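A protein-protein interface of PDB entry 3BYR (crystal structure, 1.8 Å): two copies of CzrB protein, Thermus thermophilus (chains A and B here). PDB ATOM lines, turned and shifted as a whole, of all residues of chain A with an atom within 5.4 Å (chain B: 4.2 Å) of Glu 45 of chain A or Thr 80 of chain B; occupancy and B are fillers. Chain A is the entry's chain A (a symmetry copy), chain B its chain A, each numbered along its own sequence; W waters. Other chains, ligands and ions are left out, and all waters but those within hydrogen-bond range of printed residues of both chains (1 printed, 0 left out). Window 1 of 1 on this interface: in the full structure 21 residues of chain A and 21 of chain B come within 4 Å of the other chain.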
ATOM      1  N   HIS A  31     -31.424  10.183  23.116  1.00  0.00           N
ATOM      2  CA  HIS A  31     -32.680   9.571  22.679  1.00  0.00           C
ATOM      3  C   HIS A  31     -32.498   8.144  22.126  1.00  0.00           C
ATOM      4  O   HIS A  31     -31.388   7.598  22.106  1.00  0.00           O
ATOM      5  CB  HIS A  31     -33.434  10.487  21.694  1.00  0.00           C
ATOM      6  CG  HIS A  31     -32.739  10.693  20.381  1.00  0.00           C
ATOM      7  ND1 HIS A  31     -32.397  11.943  19.911  1.00  0.00           N
ATOM      8  CD2 HIS A  31     -32.341   9.814  19.433  1.00  0.00           C
ATOM      9  CE1 HIS A  31     -31.824  11.824  18.726  1.00  0.00           C
ATOM     10  NE2 HIS A  31     -31.775  10.541  18.415  1.00  0.00           N
ATOM     11  N   ASP A  32     -33.602   7.570  21.654  1.00  0.00           N
ATOM     12  CA  ASP A  32     -33.693   6.173  21.230  1.00  0.00           C
ATOM     13  C   ASP A  32     -32.998   5.193  22.184  1.00  0.00           C
ATOM     14  O   ASP A  32     -32.144   4.392  21.779  1.00  0.00           O
ATOM     15  CB  ASP A  32     -33.234   5.986  19.773  1.00  0.00           C
ATOM     16  CG  ASP A  32     -33.688   4.658  19.188  1.00  0.00           C
ATOM     17  OD1 ASP A  32     -34.759   4.153  19.598  1.00  0.00           O
ATOM     18  OD2 ASP A  32     -32.977   4.109  18.320  1.00  0.00           O
ATOM     19  N   LEU A  33     -33.377   5.256  23.457  1.00  0.00           N
ATOM     20  CA  LEU A  33     -32.853   4.316  24.454  1.00  0.00           C
ATOM     21  C   LEU A  33     -33.422   2.926  24.194  1.00  0.00           C
ATOM     22  O   LEU A  33     -34.633   2.741  24.126  1.00  0.00           O
ATOM     23  CB  LEU A  33     -33.150   4.790  25.880  1.00  0.00           C
ATOM     24  CG  LEU A  33     -32.132   5.775  26.483  1.00  0.00           C
ATOM     25  CD1 LEU A  33     -32.127   7.119  25.748  1.00  0.00           C
ATOM     26  CD2 LEU A  33     -32.387   5.971  27.962  1.00  0.00           C
ATOM     27  N   LYS A  34     -32.535   1.958  24.006  1.00  0.00           N
ATOM     28  CA  LYS A  34     -32.946   0.586  23.772  1.00  0.00           C
ATOM     29  C   LYS A  34     -32.141  -0.304  24.692  1.00  0.00           C
ATOM     30  O   LYS A  34     -30.910  -0.270  24.688  1.00  0.00           O
ATOM     31  CB  LYS A  34     -32.745   0.188  22.315  1.00  0.00           C
ATOM     32  CG  LYS A  34     -33.754   0.829  21.347  1.00  0.00           C
ATOM     33  CD  LYS A  34     -33.488   0.414  19.917  1.00  0.00           C
ATOM     34  CE  LYS A  34     -33.550  -1.097  19.752  1.00  0.00           C
ATOM     35  NZ  LYS A  34     -34.014  -1.451  18.389  1.00  0.00           N
ATOM     36  N   THR A  35     -32.852  -1.080  25.498  1.00  0.00           N
ATOM     37  CA  THR A  35     -32.214  -1.885  26.531  1.00  0.00           C
ATOM     38  C   THR A  35     -32.565  -3.367  26.427  1.00  0.00           C
ATOM     39  O   THR A  35     -33.492  -3.753  25.716  1.00  0.00           O
ATOM     40  CB  THR A  35     -32.585  -1.407  27.943  1.00  0.00           C
ATOM     41  OG1 THR A  35     -33.993  -1.563  28.152  1.00  0.00           O
ATOM     42  CG2 THR A  35     -32.177   0.058  28.187  1.00  0.00           C
ATOM     43  N   PHE A  43     -27.674  -4.364  28.768  1.00  0.00           N
ATOM     44  CA  PHE A  43     -27.206  -3.599  27.616  1.00  0.00           C
ATOM     45  C   PHE A  43     -28.074  -2.386  27.393  1.00  0.00           C
ATOM     46  O   PHE A  43     -29.292  -2.455  27.517  1.00  0.00           O
ATOM     47  CB  PHE A  43     -27.262  -4.453  26.353  1.00  0.00           C
ATOM     48  CG  PHE A  43     -26.417  -5.677  26.418  1.00  0.00           C
ATOM     49  CD1 PHE A  43     -26.891  -6.833  27.036  1.00  0.00           C
ATOM     50  CD2 PHE A  43     -25.135  -5.674  25.895  1.00  0.00           C
ATOM     51  CE1 PHE A  43     -26.103  -7.971  27.115  1.00  0.00           C
ATOM     52  CE2 PHE A  43     -24.346  -6.814  25.956  1.00  0.00           C
ATOM     53  CZ  PHE A  43     -24.830  -7.964  26.571  1.00  0.00           C
ATOM     54  N   LEU A  44     -27.427  -1.287  27.037  1.00  0.00           N
ATOM     55  CA  LEU A  44     -28.086  -0.067  26.651  1.00  0.00           C
ATOM     56  C   LEU A  44     -27.467   0.431  25.360  1.00  0.00           C
ATOM     57  O   LEU A  44     -26.248   0.505  25.231  1.00  0.00           O
ATOM     58  CB  LEU A  44     -27.894   0.986  27.739  1.00  0.00           C
ATOM     59  CG  LEU A  44     -28.305   2.431  27.455  1.00  0.00           C
ATOM     60  CD1 LEU A  44     -29.819   2.555  27.309  1.00  0.00           C
ATOM     61  CD2 LEU A  44     -27.772   3.281  28.608  1.00  0.00           C
ATOM     62  N   GLU A  45     -28.305   0.769  24.395  1.00  0.00           N
ATOM     63  CA  GLU A  45     -27.819   1.605  23.316  1.00  0.00           C
ATOM     64  C   GLU A  45     -28.649   2.871  23.231  1.00  0.00           C
ATOM     65  O   GLU A  45     -29.867   2.860  23.455  1.00  0.00           O
ATOM     66  CB  GLU A  45     -27.757   0.868  21.983  1.00  0.00           C
ATOM     67  CG  GLU A  45     -29.079   0.340  21.480  1.00  0.00           C
ATOM     68  CD  GLU A  45     -29.013  -0.062  20.028  1.00  0.00           C
ATOM     69  OE1 GLU A  45     -28.214  -0.974  19.689  1.00  0.00           O
ATOM     70  OE2 GLU A  45     -29.761   0.535  19.225  1.00  0.00           O
ATOM     71  N   PHE A  46     -27.974   3.975  22.951  1.00  0.00           N
ATOM     72  CA  PHE A  46     -28.676   5.235  22.772  1.00  0.00           C
ATOM     73  C   PHE A  46     -27.945   6.164  21.818  1.00  0.00           C
ATOM     74  O   PHE A  46     -26.814   5.901  21.408  1.00  0.00           O
ATOM     75  CB  PHE A  46     -28.987   5.908  24.121  1.00  0.00           C
ATOM     76  CG  PHE A  46     -27.771   6.332  24.900  1.00  0.00           C
ATOM     77  CD1 PHE A  46     -27.317   7.650  24.839  1.00  0.00           C
ATOM     78  CD2 PHE A  46     -27.102   5.425  25.721  1.00  0.00           C
ATOM     79  CE1 PHE A  46     -26.199   8.055  25.566  1.00  0.00           C
ATOM     80  CE2 PHE A  46     -25.980   5.808  26.445  1.00  0.00           C
ATOM     81  CZ  PHE A  46     -25.529   7.130  26.380  1.00  0.00           C
ATOM     82  N   HIS A  47     -28.631   7.245  21.461  1.00  0.00           N
ATOM     83  CA  HIS A  47     -28.097   8.268  20.597  1.00  0.00           C
ATOM     84  C   HIS A  47     -27.762   9.474  21.451  1.00  0.00           C
ATOM     85  O   HIS A  47     -28.580   9.925  22.265  1.00  0.00           O
ATOM     86  CB  HIS A  47     -29.123   8.667  19.547  1.00  0.00           C
ATOM     87  CG  HIS A  47     -29.514   7.561  18.619  1.00  0.00           C
ATOM     88  ND1 HIS A  47     -30.281   7.782  17.497  1.00  0.00           N
ATOM     89  CD2 HIS A  47     -29.236   6.234  18.628  1.00  0.00           C
ATOM     90  CE1 HIS A  47     -30.479   6.639  16.866  1.00  0.00           C
ATOM     91  NE2 HIS A  47     -29.843   5.688  17.523  1.00  0.00           N
ATOM     92  N   ALA A  79     -22.974   0.174  27.948  1.00  0.00           N
ATOM     93  CA  ALA A  79     -23.607   1.060  26.963  1.00  0.00           C
ATOM     94  C   ALA A  79     -22.825   1.177  25.652  1.00  0.00           C
ATOM     95  O   ALA A  79     -21.587   1.244  25.663  1.00  0.00           O
ATOM     96  CB  ALA A  79     -23.829   2.433  27.567  1.00  0.00           C
ATOM     97  N   THR A  80     -23.560   1.185  24.539  1.00  0.00           N
ATOM     98  CA  THR A  80     -23.032   1.530  23.215  1.00  0.00           C
ATOM     99  C   THR A  80     -23.679   2.843  22.787  1.00  0.00           C
ATOM    100  O   THR A  80     -24.905   2.956  22.762  1.00  0.00           O
ATOM    101  CB  THR A  80     -23.332   0.432  22.160  1.00  0.00           C
ATOM    102  OG1 THR A  80     -22.956  -0.837  22.689  1.00  0.00           O
ATOM    103  CG2 THR A  80     -22.549   0.674  20.855  1.00  0.00           C
ATOM    104  N   HIS A  82     -24.210   5.983  20.103  1.00  0.00           N
ATOM    105  CA  HIS A  82     -24.183   6.468  18.727  1.00  0.00           C
ATOM    106  C   HIS A  82     -24.302   7.989  18.746  1.00  0.00           C
ATOM    107  O   HIS A  82     -25.334   8.534  19.169  1.00  0.00           O
ATOM    108  CB  HIS A  82     -25.322   5.821  17.932  1.00  0.00           C
ATOM    109  CG  HIS A  82     -25.536   6.409  16.569  1.00  0.00           C
ATOM    110  ND1 HIS A  82     -24.570   6.379  15.586  1.00  0.00           N
ATOM    111  CD2 HIS A  82     -26.610   7.027  16.019  1.00  0.00           C
ATOM    112  CE1 HIS A  82     -25.030   6.969  14.499  1.00  0.00           C
ATOM    113  NE2 HIS A  82     -26.270   7.361  14.731  1.00  0.00           N
ATOM    114  N   LEU B  44     -26.587  -5.596  14.639  1.00  0.00           N
ATOM    115  CA  LEU B  44     -25.158  -5.440  14.598  1.00  0.00           C
ATOM    116  C   LEU B  44     -24.787  -4.172  15.342  1.00  0.00           C
ATOM    117  O   LEU B  44     -25.372  -3.116  15.121  1.00  0.00           O
ATOM    118  CB  LEU B  44     -24.695  -5.324  13.148  1.00  0.00           C
ATOM    119  CG  LEU B  44     -23.249  -4.922  12.860  1.00  0.00           C
ATOM    120  CD1 LEU B  44     -22.274  -6.009  13.305  1.00  0.00           C
ATOM    121  CD2 LEU B  44     -23.151  -4.649  11.360  1.00  0.00           C
ATOM    122  N   GLU B  45     -23.816  -4.274  16.234  1.00  0.00           N
ATOM    123  CA  GLU B  45     -23.155  -3.063  16.680  1.00  0.00           C
ATOM    124  C   GLU B  45     -21.668  -3.156  16.401  1.00  0.00           C
ATOM    125  O   GLU B  45     -21.056  -4.227  16.512  1.00  0.00           O
ATOM    126  CB  GLU B  45     -23.448  -2.736  18.139  1.00  0.00           C
ATOM    127  CG  GLU B  45     -23.011  -3.788  19.131  1.00  0.00           C
ATOM    128  CD  GLU B  45     -23.009  -3.266  20.547  1.00  0.00           C
ATOM    129  OE1 GLU B  45     -24.094  -2.864  21.043  1.00  0.00           O
ATOM    130  OE2 GLU B  45     -21.923  -3.258  21.162  1.00  0.00           O
ATOM    131  N   PHE B  46     -21.096  -2.034  15.992  1.00  0.00           N
ATOM    132  CA  PHE B  46     -19.661  -1.986  15.766  1.00  0.00           C
ATOM    133  C   PHE B  46     -19.092  -0.597  16.002  1.00  0.00           C
ATOM    134  O   PHE B  46     -19.829   0.372  16.194  1.00  0.00           O
ATOM    135  CB  PHE B  46     -19.285  -2.545  14.381  1.00  0.00           C
ATOM    136  CG  PHE B  46     -19.814  -1.742  13.223  1.00  0.00           C
ATOM    137  CD1 PHE B  46     -19.003  -0.803  12.585  1.00  0.00           C
ATOM    138  CD2 PHE B  46     -21.108  -1.950  12.748  1.00  0.00           C
ATOM    139  CE1 PHE B  46     -19.481  -0.064  11.504  1.00  0.00           C
ATOM    140  CE2 PHE B  46     -21.604  -1.216  11.677  1.00  0.00           C
ATOM    141  CZ  PHE B  46     -20.788  -0.276  11.042  1.00  0.00           C
ATOM    142  N   ALA B  79     -28.120  -1.845  12.113  1.00  0.00           N
ATOM    143  CA  ALA B  79     -26.822  -1.545  12.731  1.00  0.00           C
ATOM    144  C   ALA B  79     -26.840  -0.298  13.620  1.00  0.00           C
ATOM    145  O   ALA B  79     -27.476   0.709  13.277  1.00  0.00           O
ATOM    146  CB  ALA B  79     -25.756  -1.412  11.661  1.00  0.00           C
ATOM    147  N   THR B  80     -26.151  -0.390  14.759  1.00  0.00           N
ATOM    148  CA  THR B  80     -25.845   0.756  15.621  1.00  0.00           C
ATOM    149  C   THR B  80     -24.337   0.979  15.574  1.00  0.00           C
ATOM    150  O   THR B  80     -23.561   0.062  15.848  1.00  0.00           O
ATOM    151  CB  THR B  80     -26.292   0.520  17.090  1.00  0.00           C
ATOM    152  OG1 THR B  80     -27.639   0.057  17.097  1.00  0.00           O
ATOM    153  CG2 THR B  80     -26.212   1.817  17.918  1.00  0.00           C
ATOM    154  N   ILE B  81     -23.929   2.192  15.219  1.00  0.00           N
ATOM    155  CA  ILE B  81     -22.521   2.485  14.983  1.00  0.00           C
ATOM    156  C   ILE B  81     -21.984   3.453  16.013  1.00  0.00           C
ATOM    157  O   ILE B  81     -22.560   4.522  16.238  1.00  0.00           O
ATOM    158  CB  ILE B  81     -22.292   3.035  13.551  1.00  0.00           C
ATOM    159  CG1 ILE B  81     -22.956   2.100  12.530  1.00  0.00           C
ATOM    160  CG2 ILE B  81     -20.794   3.231  13.278  1.00  0.00           C
ATOM    161  CD1 ILE B  81     -23.015   2.648  11.110  1.00  0.00           C
ATOM    162  N   HIS B  82     -20.886   3.049  16.645  1.00  0.00           N
ATOM    163  CA  HIS B  82     -20.176   3.877  17.614  1.00  0.00           C
ATOM    164  C   HIS B  82     -18.906   4.411  16.958  1.00  0.00           C
ATOM    165  O   HIS B  82     -18.005   3.634  16.608  1.00  0.00           O
ATOM    166  CB  HIS B  82     -19.863   3.051  18.866  1.00  0.00           C
ATOM    167  CG  HIS B  82     -18.942   3.726  19.838  1.00  0.00           C
ATOM    168  ND1 HIS B  82     -19.260   4.913  20.462  1.00  0.00           N
ATOM    169  CD2 HIS B  82     -17.720   3.372  20.305  1.00  0.00           C
ATOM    170  CE1 HIS B  82     -18.268   5.271  21.256  1.00  0.00           C
ATOM    171  NE2 HIS B  82     -17.326   4.347  21.188  1.00  0.00           N
HETATM  172  O   HOH W   1     -26.186   3.869  14.356  1.00  0.00           O
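Glu 45 of chain A touches Thr 80 of chain B, and with the chains exchanged Thr 80 of chain A touches Glu 45 of chain B.
Positions printed for both chains: 44, 45, 46, 79, 80 and 82.
Of the 3 pairs that touch across the chains among the printed residues, 2 have their exchanged pair printed and touching as well.
Of the printed residues of chain B, His 82 of chain A touches Ile 81.
Of the printed residues of chain A, Glu 45 of chain B touches Thr 80.
Of the printed residues of chain B, Thr 80 of chain A touches Glu 45 (2.8 Å).
Of the printed residues of chain A, Ile 81 of chain B touches His 82 (2.8 Å).
Leu 44 of chain B touches none of the printed residues of chain A.
The nearest printed residue of chain B that does not touch Glu 45 of chain A is Glu 45 of chain B (4.7 Å).
Water W1 bridges N of Ile 81 of chain B (2.9 Å) and ND1 of His 82 of chain A (3.2 Å).
Of the 13 printed residues of chain A, 3 touch a printed residue of chain B.
Printed residues of chain A that touch a printed residue of chain B: Glu 45, Thr 80 and His 82.
Along chain B the printed residues that touch a printed residue of chain A span positions 45 to 81.
Among the printed residues, 3 pairs touch across the chains.
Among the printed residues, no Asp or Glu carboxylate lies within 4 Å of a Lys or Arg side-chain nitrogen of the other chain.
The side-chain carboxylate (OE1) of Glu 45 of chain B is in hydrogen-bond range of the side-chain hydroxyl (OG1) of Thr 80 of chain A (2.8 Å).
The side-chain carboxylate of Glu 45 of chain A sits at hydrogen-bond distance from the side-chain hydroxyl of Thr 80 of chain B, at 2.8 Å.
The backbone carbonyl oxygen (O) of Ile 81 of chain B lies within hydrogen-bond range of a ring nitrogen (ND1) of His 82 of chain A (2.8 Å).
The backbone carbonyl oxygen of Leu 44 of chain B is in hydrogen-bond range of the backbone NH of Thr 80 of chain B (2.9 Å).
N of Phe 46 of chain B is in hydrogen-bond range of O of Thr 80 of chain B.
O of Lys 34 of chain A sits at hydrogen-bond distance from N of Glu 45 of chain A, at 2.8 Å.
The backbone NH (N) of Thr 80 of chain A lies within hydrogen-bond range of the backbone carbonyl oxygen (O) of Leu 44 of chain A.
O of Thr 80 of chain A lies within hydrogen-bond range of N of Phe 46 of chain A (3.2 Å).
The backbone NH (N) of His 82 of chain A is in hydrogen-bond range of the backbone carbonyl oxygen (O) of Phe 46 of chain A, 2.9 Å away.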
